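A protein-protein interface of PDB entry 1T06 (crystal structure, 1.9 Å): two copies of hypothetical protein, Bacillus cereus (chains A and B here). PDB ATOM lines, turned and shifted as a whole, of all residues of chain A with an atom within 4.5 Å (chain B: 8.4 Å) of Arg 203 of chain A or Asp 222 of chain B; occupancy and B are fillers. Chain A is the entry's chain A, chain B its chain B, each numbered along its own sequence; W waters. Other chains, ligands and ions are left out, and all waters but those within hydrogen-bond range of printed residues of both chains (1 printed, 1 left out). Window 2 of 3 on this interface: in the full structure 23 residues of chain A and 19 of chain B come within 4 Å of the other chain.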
ATOM      1  N   ILE A  21      13.709   8.741 -24.862  1.00  0.00           N
ATOM      2  CA  ILE A  21      14.657   7.641 -24.741  1.00  0.00           C
ATOM      3  C   ILE A  21      14.487   6.674 -25.919  1.00  0.00           C
ATOM      4  O   ILE A  21      15.456   6.376 -26.623  1.00  0.00           O
ATOM      5  CB  ILE A  21      14.441   6.858 -23.434  1.00  0.00           C
ATOM      6  CG1 ILE A  21      14.788   7.734 -22.228  1.00  0.00           C
ATOM      7  CG2 ILE A  21      15.284   5.601 -23.445  1.00  0.00           C
ATOM      8  CD1 ILE A  21      14.385   7.120 -20.896  1.00  0.00           C
ATOM      9  N   ASN A  25      16.902   5.687 -28.961  1.00  0.00           N
ATOM     10  CA  ASN A  25      17.354   4.334 -29.273  1.00  0.00           C
ATOM     11  C   ASN A  25      17.142   3.951 -30.734  1.00  0.00           C
ATOM     12  O   ASN A  25      17.689   2.946 -31.203  1.00  0.00           O
ATOM     13  CB  ASN A  25      16.660   3.310 -28.363  1.00  0.00           C
ATOM     14  CG  ASN A  25      16.927   3.562 -26.876  1.00  0.00           C
ATOM     15  OD1 ASN A  25      17.956   4.120 -26.508  1.00  0.00           O
ATOM     16  ND2 ASN A  25      16.006   3.132 -26.020  1.00  0.00           N
ATOM     17  N   MET A  93      15.042  -2.531 -30.626  1.00  0.00           N
ATOM     18  CA  MET A  93      14.081  -2.802 -29.557  1.00  0.00           C
ATOM     19  C   MET A  93      12.976  -3.753 -30.050  1.00  0.00           C
ATOM     20  O   MET A  93      12.440  -4.556 -29.281  1.00  0.00           O
ATOM     21  CB  MET A  93      13.467  -1.497 -29.023  1.00  0.00           C
ATOM     22  CG  MET A  93      14.451  -0.597 -28.251  1.00  0.00           C
ATOM     23  SD  MET A  93      13.646   0.770 -27.396  1.00  0.00           S
ATOM     24  CE  MET A  93      13.297   0.051 -25.802  1.00  0.00           C
ATOM     25  N   ARG A 166      24.163  -3.778 -34.308  1.00  0.00           N
ATOM     26  CA  ARG A 166      23.131  -4.413 -33.513  1.00  0.00           C
ATOM     27  C   ARG A 166      23.342  -5.894 -33.298  1.00  0.00           C
ATOM     28  O   ARG A 166      22.990  -6.432 -32.251  1.00  0.00           O
ATOM     29  CB  ARG A 166      21.768  -4.136 -34.133  1.00  0.00           C
ATOM     30  CG  ARG A 166      21.245  -2.823 -33.650  1.00  0.00           C
ATOM     31  CD  ARG A 166      21.192  -2.951 -32.154  1.00  0.00           C
ATOM     32  NE  ARG A 166      21.588  -1.756 -31.440  1.00  0.00           N
ATOM     33  CZ  ARG A 166      21.731  -1.714 -30.122  1.00  0.00           C
ATOM     34  NH1 ARG A 166      21.514  -2.805 -29.393  1.00  0.00           N
ATOM     35  NH2 ARG A 166      22.075  -0.584 -29.532  1.00  0.00           N
ATOM     36  N   VAL A 201      29.500  -1.243 -29.382  1.00  0.00           N
ATOM     37  CA  VAL A 201      28.304  -1.148 -30.207  1.00  0.00           C
ATOM     38  C   VAL A 201      28.112   0.338 -30.495  1.00  0.00           C
ATOM     39  O   VAL A 201      27.753   1.122 -29.614  1.00  0.00           O
ATOM     40  CB  VAL A 201      27.046  -1.697 -29.479  1.00  0.00           C
ATOM     41  CG1 VAL A 201      25.813  -1.507 -30.363  1.00  0.00           C
ATOM     42  CG2 VAL A 201      27.232  -3.176 -29.158  1.00  0.00           C
ATOM     43  N   LYS A 202      28.366   0.721 -31.739  1.00  0.00           N
ATOM     44  CA  LYS A 202      28.244   2.109 -32.146  1.00  0.00           C
ATOM     45  C   LYS A 202      26.780   2.489 -32.319  1.00  0.00           C
ATOM     46  O   LYS A 202      26.000   1.746 -32.917  1.00  0.00           O
ATOM     47  CB  LYS A 202      29.049   2.313 -33.427  1.00  0.00           C
ATOM     48  CG  LYS A 202      30.492   1.832 -33.232  1.00  0.00           C
ATOM     49  CD  LYS A 202      31.236   1.637 -34.528  1.00  0.00           C
ATOM     50  CE  LYS A 202      32.610   1.046 -34.265  1.00  0.00           C
ATOM     51  NZ  LYS A 202      33.444   0.979 -35.506  1.00  0.00           N
ATOM     52  N   ARG A 203      26.414   3.640 -31.761  1.00  0.00           N
ATOM     53  CA  ARG A 203      25.043   4.131 -31.819  1.00  0.00           C
ATOM     54  C   ARG A 203      24.980   5.524 -32.436  1.00  0.00           C
ATOM     55  O   ARG A 203      25.907   6.321 -32.292  1.00  0.00           O
ATOM     56  CB  ARG A 203      24.443   4.150 -30.410  1.00  0.00           C
ATOM     57  CG  ARG A 203      24.471   2.789 -29.730  1.00  0.00           C
ATOM     58  CD  ARG A 203      23.738   2.797 -28.399  1.00  0.00           C
ATOM     59  NE  ARG A 203      24.439   3.564 -27.373  1.00  0.00           N
ATOM     60  CZ  ARG A 203      24.043   3.654 -26.107  1.00  0.00           C
ATOM     61  NH1 ARG A 203      22.947   3.028 -25.700  1.00  0.00           N
ATOM     62  NH2 ARG A 203      24.752   4.362 -25.242  1.00  0.00           N
ATOM     63  N   ASP A 204      23.880   5.808 -33.127  1.00  0.00           N
ATOM     64  CA  ASP A 204      23.686   7.100 -33.777  1.00  0.00           C
ATOM     65  C   ASP A 204      23.491   8.255 -32.811  1.00  0.00           C
ATOM     66  O   ASP A 204      22.605   8.225 -31.955  1.00  0.00           O
ATOM     67  CB  ASP A 204      22.485   7.038 -34.724  1.00  0.00           C
ATOM     68  CG  ASP A 204      22.888   6.743 -36.161  1.00  0.00           C
ATOM     69  OD1 ASP A 204      23.682   5.797 -36.380  1.00  0.00           O
ATOM     70  OD2 ASP A 204      22.402   7.459 -37.070  1.00  0.00           O
ATOM     71  N   ASN A 205      24.335   9.272 -32.962  1.00  0.00           N
ATOM     72  CA  ASN A 205      24.269  10.476 -32.143  1.00  0.00           C
ATOM     73  C   ASN A 205      24.280  10.252 -30.639  1.00  0.00           C
ATOM     74  O   ASN A 205      23.521  10.888 -29.907  1.00  0.00           O
ATOM     75  CB  ASN A 205      23.026  11.291 -32.514  1.00  0.00           C
ATOM     76  CG  ASN A 205      22.988  11.650 -33.985  1.00  0.00           C
ATOM     77  OD1 ASN A 205      23.953  12.197 -34.529  1.00  0.00           O
ATOM     78  ND2 ASN A 205      21.872  11.348 -34.640  1.00  0.00           N
ATOM     79  N   LYS A 206      25.132   9.347 -30.177  1.00  0.00           N
ATOM     80  CA  LYS A 206      25.255   9.076 -28.749  1.00  0.00           C
ATOM     81  C   LYS A 206      26.462   8.191 -28.532  1.00  0.00           C
ATOM     82  O   LYS A 206      26.912   7.512 -29.455  1.00  0.00           O
ATOM     83  CB  LYS A 206      23.983   8.414 -28.196  1.00  0.00           C
ATOM     84  CG  LYS A 206      23.634   7.067 -28.800  1.00  0.00           C
ATOM     85  CD  LYS A 206      22.198   6.665 -28.457  1.00  0.00           C
ATOM     86  CE  LYS A 206      21.967   6.574 -26.958  1.00  0.00           C
ATOM     87  NZ  LYS A 206      20.571   6.165 -26.626  1.00  0.00           N
ATOM     88  N   LYS A 207      27.003   8.224 -27.320  1.00  0.00           N
ATOM     89  CA  LYS A 207      28.173   7.423 -26.991  1.00  0.00           C
ATOM     90  C   LYS A 207      27.893   5.950 -27.271  1.00  0.00           C
ATOM     91  O   LYS A 207      26.801   5.450 -26.986  1.00  0.00           O
ATOM     92  CB  LYS A 207      28.529   7.611 -25.519  1.00  0.00           C
ATOM     93  CG  LYS A 207      28.823   9.052 -25.127  1.00  0.00           C
ATOM     94  CD  LYS A 207      28.861   9.211 -23.605  1.00  0.00           C
ATOM     95  CE  LYS A 207      29.286  10.613 -23.195  1.00  0.00           C
ATOM     96  NZ  LYS A 207      30.684  10.911 -23.627  1.00  0.00           N
ATOM     97  N   SER A 208      28.870   5.256 -27.842  1.00  0.00           N
ATOM     98  CA  SER A 208      28.685   3.847 -28.144  1.00  0.00           C
ATOM     99  C   SER A 208      28.620   3.033 -26.853  1.00  0.00           C
ATOM    100  O   SER A 208      29.115   3.463 -25.816  1.00  0.00           O
ATOM    101  CB  SER A 208      29.821   3.345 -29.047  1.00  0.00           C
ATOM    102  OG  SER A 208      31.085   3.551 -28.451  1.00  0.00           O
ATOM    103  N   SER A 209      27.983   1.867 -26.920  1.00  0.00           N
ATOM    104  CA  SER A 209      27.871   0.980 -25.767  1.00  0.00           C
ATOM    105  C   SER A 209      29.119   0.119 -25.701  1.00  0.00           C
ATOM    106  O   SER A 209      29.435  -0.602 -26.647  1.00  0.00           O
ATOM    107  CB  SER A 209      26.655   0.057 -25.893  1.00  0.00           C
ATOM    108  OG  SER A 209      25.439   0.782 -25.856  1.00  0.00           O
ATOM    109  N   ILE B 180      15.308   3.631 -10.572  1.00  0.00           N
ATOM    110  CA  ILE B 180      14.399   2.906 -11.455  1.00  0.00           C
ATOM    111  C   ILE B 180      13.053   2.491 -10.842  1.00  0.00           C
ATOM    112  O   ILE B 180      12.017   2.607 -11.494  1.00  0.00           O
ATOM    113  CB  ILE B 180      15.084   1.634 -12.033  1.00  0.00           C
ATOM    114  CG1 ILE B 180      16.295   2.032 -12.883  1.00  0.00           C
ATOM    115  CG2 ILE B 180      14.102   0.833 -12.871  1.00  0.00           C
ATOM    116  CD1 ILE B 180      15.964   2.926 -14.054  1.00  0.00           C
ATOM    117  N   GLU B 215      25.754   4.562 -15.063  1.00  0.00           N
ATOM    118  CA  GLU B 215      25.612   3.779 -16.283  1.00  0.00           C
ATOM    119  C   GLU B 215      24.537   2.706 -16.163  1.00  0.00           C
ATOM    120  O   GLU B 215      23.721   2.542 -17.067  1.00  0.00           O
ATOM    121  CB  GLU B 215      26.945   3.139 -16.667  1.00  0.00           C
ATOM    122  CG  GLU B 215      27.582   3.791 -17.877  1.00  0.00           C
ATOM    123  CD  GLU B 215      28.933   3.192 -18.216  1.00  0.00           C
ATOM    124  OE1 GLU B 215      29.021   1.948 -18.358  1.00  0.00           O
ATOM    125  OE2 GLU B 215      29.907   3.969 -18.344  1.00  0.00           O
ATOM    126  N   SER B 216      24.538   1.978 -15.053  1.00  0.00           N
ATOM    127  CA  SER B 216      23.535   0.942 -14.837  1.00  0.00           C
ATOM    128  C   SER B 216      22.127   1.535 -14.943  1.00  0.00           C
ATOM    129  O   SER B 216      21.270   1.017 -15.669  1.00  0.00           O
ATOM    130  CB  SER B 216      23.732   0.307 -13.463  1.00  0.00           C
ATOM    131  OG  SER B 216      24.963  -0.386 -13.430  1.00  0.00           O
ATOM    132  N   ILE B 217      21.893   2.622 -14.215  1.00  0.00           N
ATOM    133  CA  ILE B 217      20.599   3.292 -14.242  1.00  0.00           C
ATOM    134  C   ILE B 217      20.247   3.641 -15.684  1.00  0.00           C
ATOM    135  O   ILE B 217      19.093   3.505 -16.103  1.00  0.00           O
ATOM    136  CB  ILE B 217      20.625   4.604 -13.420  1.00  0.00           C
ATOM    137  CG1 ILE B 217      20.771   4.289 -11.930  1.00  0.00           C
ATOM    138  CG2 ILE B 217      19.352   5.409 -13.676  1.00  0.00           C
ATOM    139  CD1 ILE B 217      20.965   5.518 -11.080  1.00  0.00           C
ATOM    140  N   GLN B 218      21.249   4.090 -16.436  1.00  0.00           N
ATOM    141  CA  GLN B 218      21.054   4.472 -17.830  1.00  0.00           C
ATOM    142  C   GLN B 218      20.651   3.265 -18.684  1.00  0.00           C
ATOM    143  O   GLN B 218      19.719   3.354 -19.484  1.00  0.00           O
ATOM    144  CB  GLN B 218      22.333   5.115 -18.377  1.00  0.00           C
ATOM    145  CG  GLN B 218      22.143   5.907 -19.661  1.00  0.00           C
ATOM    146  CD  GLN B 218      21.053   6.963 -19.555  1.00  0.00           C
ATOM    147  OE1 GLN B 218      19.959   6.792 -20.094  1.00  0.00           O
ATOM    148  NE2 GLN B 218      21.344   8.056 -18.861  1.00  0.00           N
ATOM    149  N   LYS B 219      21.339   2.140 -18.510  1.00  0.00           N
ATOM    150  CA  LYS B 219      20.998   0.938 -19.265  1.00  0.00           C
ATOM    151  C   LYS B 219      19.549   0.522 -19.002  1.00  0.00           C
ATOM    152  O   LYS B 219      18.848   0.090 -19.915  1.00  0.00           O
ATOM    153  CB  LYS B 219      21.942  -0.208 -18.909  1.00  0.00           C
ATOM    154  CG  LYS B 219      23.354  -0.013 -19.415  1.00  0.00           C
ATOM    155  CD  LYS B 219      24.236  -1.143 -18.941  1.00  0.00           C
ATOM    156  CE  LYS B 219      25.700  -0.858 -19.212  1.00  0.00           C
ATOM    157  NZ  LYS B 219      26.575  -1.816 -18.464  1.00  0.00           N
ATOM    158  N   GLU B 220      19.099   0.649 -17.758  1.00  0.00           N
ATOM    159  CA  GLU B 220      17.718   0.302 -17.431  1.00  0.00           C
ATOM    160  C   GLU B 220      16.740   1.254 -18.117  1.00  0.00           C
ATOM    161  O   GLU B 220      15.732   0.818 -18.676  1.00  0.00           O
ATOM    162  CB  GLU B 220      17.509   0.324 -15.919  1.00  0.00           C
ATOM    163  CG  GLU B 220      18.255  -0.786 -15.224  1.00  0.00           C
ATOM    164  CD  GLU B 220      17.953  -2.143 -15.843  1.00  0.00           C
ATOM    165  OE1 GLU B 220      16.821  -2.647 -15.660  1.00  0.00           O
ATOM    166  OE2 GLU B 220      18.850  -2.699 -16.522  1.00  0.00           O
ATOM    167  N   LEU B 221      17.043   2.551 -18.073  1.00  0.00           N
ATOM    168  CA  LEU B 221      16.205   3.557 -18.717  1.00  0.00           C
ATOM    169  C   LEU B 221      16.130   3.279 -20.215  1.00  0.00           C
ATOM    170  O   LEU B 221      15.055   3.375 -20.817  1.00  0.00           O
ATOM    171  CB  LEU B 221      16.774   4.964 -18.519  1.00  0.00           C
ATOM    172  CG  LEU B 221      16.709   5.622 -17.141  1.00  0.00           C
ATOM    173  CD1 LEU B 221      17.269   7.045 -17.243  1.00  0.00           C
ATOM    174  CD2 LEU B 221      15.266   5.648 -16.643  1.00  0.00           C
ATOM    175  N   ASP B 222      17.271   2.937 -20.812  1.00  0.00           N
ATOM    176  CA  ASP B 222      17.329   2.653 -22.241  1.00  0.00           C
ATOM    177  C   ASP B 222      16.341   1.584 -22.664  1.00  0.00           C
ATOM    178  O   ASP B 222      15.755   1.663 -23.748  1.00  0.00           O
ATOM    179  CB  ASP B 222      18.736   2.210 -22.650  1.00  0.00           C
ATOM    180  CG  ASP B 222      19.709   3.362 -22.718  1.00  0.00           C
ATOM    181  OD1 ASP B 222      19.264   4.531 -22.604  1.00  0.00           O
ATOM    182  OD2 ASP B 222      20.919   3.098 -22.891  1.00  0.00           O
ATOM    183  N   ARG B 223      16.159   0.584 -21.807  1.00  0.00           N
ATOM    184  CA  ARG B 223      15.255  -0.527 -22.086  1.00  0.00           C
ATOM    185  C   ARG B 223      13.795  -0.191 -21.752  1.00  0.00           C
ATOM    186  O   ARG B 223      12.891  -0.991 -21.997  1.00  0.00           O
ATOM    187  CB  ARG B 223      15.709  -1.749 -21.288  1.00  0.00           C
ATOM    188  CG  ARG B 223      14.911  -3.015 -21.519  1.00  0.00           C
ATOM    189  CD  ARG B 223      15.354  -4.077 -20.517  1.00  0.00           C
ATOM    190  NE  ARG B 223      16.799  -4.303 -20.588  1.00  0.00           N
ATOM    191  CZ  ARG B 223      17.388  -5.141 -21.438  1.00  0.00           C
ATOM    192  NH1 ARG B 223      16.659  -5.849 -22.295  1.00  0.00           N
ATOM    193  NH2 ARG B 223      18.709  -5.260 -21.442  1.00  0.00           N
ATOM    194  N   GLY B 224      13.567   0.993 -21.196  1.00  0.00           N
ATOM    195  CA  GLY B 224      12.215   1.397 -20.844  1.00  0.00           C
ATOM    196  C   GLY B 224      11.759   0.802 -19.527  1.00  0.00           C
ATOM    197  O   GLY B 224      10.574   0.505 -19.353  1.00  0.00           O
ATOM    198  N   ARG B 225      12.706   0.639 -18.599  1.00  0.00           N
ATOM    199  CA  ARG B 225      12.426   0.069 -17.281  1.00  0.00           C
ATOM    200  C   ARG B 225      12.138   1.115 -16.219  1.00  0.00           C
ATOM    201  O   ARG B 225      12.042   0.784 -15.043  1.00  0.00           O
ATOM    202  CB  ARG B 225      13.591  -0.795 -16.798  1.00  0.00           C
ATOM    203  CG  ARG B 225      13.866  -2.047 -17.618  1.00  0.00           C
ATOM    204  CD  ARG B 225      12.729  -3.056 -17.554  1.00  0.00           C
ATOM    205  NE  ARG B 225      13.156  -4.342 -18.111  1.00  0.00           N
ATOM    206  CZ  ARG B 225      12.344  -5.355 -18.412  1.00  0.00           C
ATOM    207  NH1 ARG B 225      11.034  -5.245 -18.216  1.00  0.00           N
ATOM    208  NH2 ARG B 225      12.845  -6.478 -18.919  1.00  0.00           N
ATOM    209  N   LEU B 226      12.009   2.372 -16.609  1.00  0.00           N
ATOM    210  CA  LEU B 226      11.706   3.387 -15.615  1.00  0.00           C
ATOM    211  C   LEU B 226      10.411   2.995 -14.906  1.00  0.00           C
ATOM    212  O   LEU B 226       9.439   2.599 -15.550  1.00  0.00           O
ATOM    213  CB  LEU B 226      11.532   4.757 -16.261  1.00  0.00           C
ATOM    214  CG  LEU B 226      11.227   5.840 -15.220  1.00  0.00           C
ATOM    215  CD1 LEU B 226      12.429   6.015 -14.297  1.00  0.00           C
ATOM    216  CD2 LEU B 226      10.882   7.147 -15.914  1.00  0.00           C
HETATM  217  O   HOH W   1      21.292   6.088 -23.918  1.00  0.00           O
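Arg 203 of chain A touches one residue of chain B.
Asp 222 of chain B touches just these residues of chain A: Ile 21, Asn 25, Met 93 and Arg 203.
Of the printed residues of chain B, Ile 21 of chain A touches Leu 221 and Asp 222.
Of the printed residues of chain A, Leu 221 of chain B touches Ile 21 (3.5 Å).
Gln 218 of chain B touches none of the printed residues of chain A.
The nearest residue of chain B that does not touch Arg 203 of chain A is Gln 218 of chain B (6.4 Å).
The nearest printed residue of chain A that does not touch Asp 222 of chain B is Lys 206 of chain A (4.5 Å).
The side-chain amide nitrogen (ND2) of Asn 25 of chain A sits at hydrogen-bond distance from the backbone carbonyl oxygen (O) of Asp 222 of chain B (2.7 Å).
NH1 of Arg 203 of chain A lies within salt-bridge range of OD2 of Asp 222 of chain B (3.5 Å).
Water W1 lies within hydrogen-bond range of NZ of Lys 206 of chain A (2.8 Å) and OD1 of Asp 222 of chain B (2.9 Å).
O of Ile 21 of chain A sits close to ND2 of Asn 25 of chain A (3.3 Å).
The side-chain amide nitrogen (ND2) of Asn 25 of chain A lies within hydrogen-bond range of the side-chain sulfur (SD) of Met 93 of chain A (3.6 Å).
OD1 of Asn 25 of chain A is in hydrogen-bond range of NZ of Lys 206 of chain A (3.3 Å).
The guanidinium group (NH2) of Arg 203 of chain A lies within hydrogen-bond range of the backbone carbonyl oxygen (O) of Lys 207 of chain A, 2.9 Å away.
OG of Ser 209 of chain A sits close to NE of Arg 203 of chain A.
The side-chain amide oxygen (OE1) of Gln 218 of chain B sits close to the side-chain carboxylate (OD1) of Asp 222 of chain B (3.4 Å).
Among the printed residues, merely in contact across the chains: Ile 21 of chain A with Leu 221 of chain B, Ile 21 of chain A with Asp 222 of chain B, Met 93 of chain A with Asp 222 of chain B and Met 93 of chain A with Arg 223 of chain B.
No position is printed for both chains.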
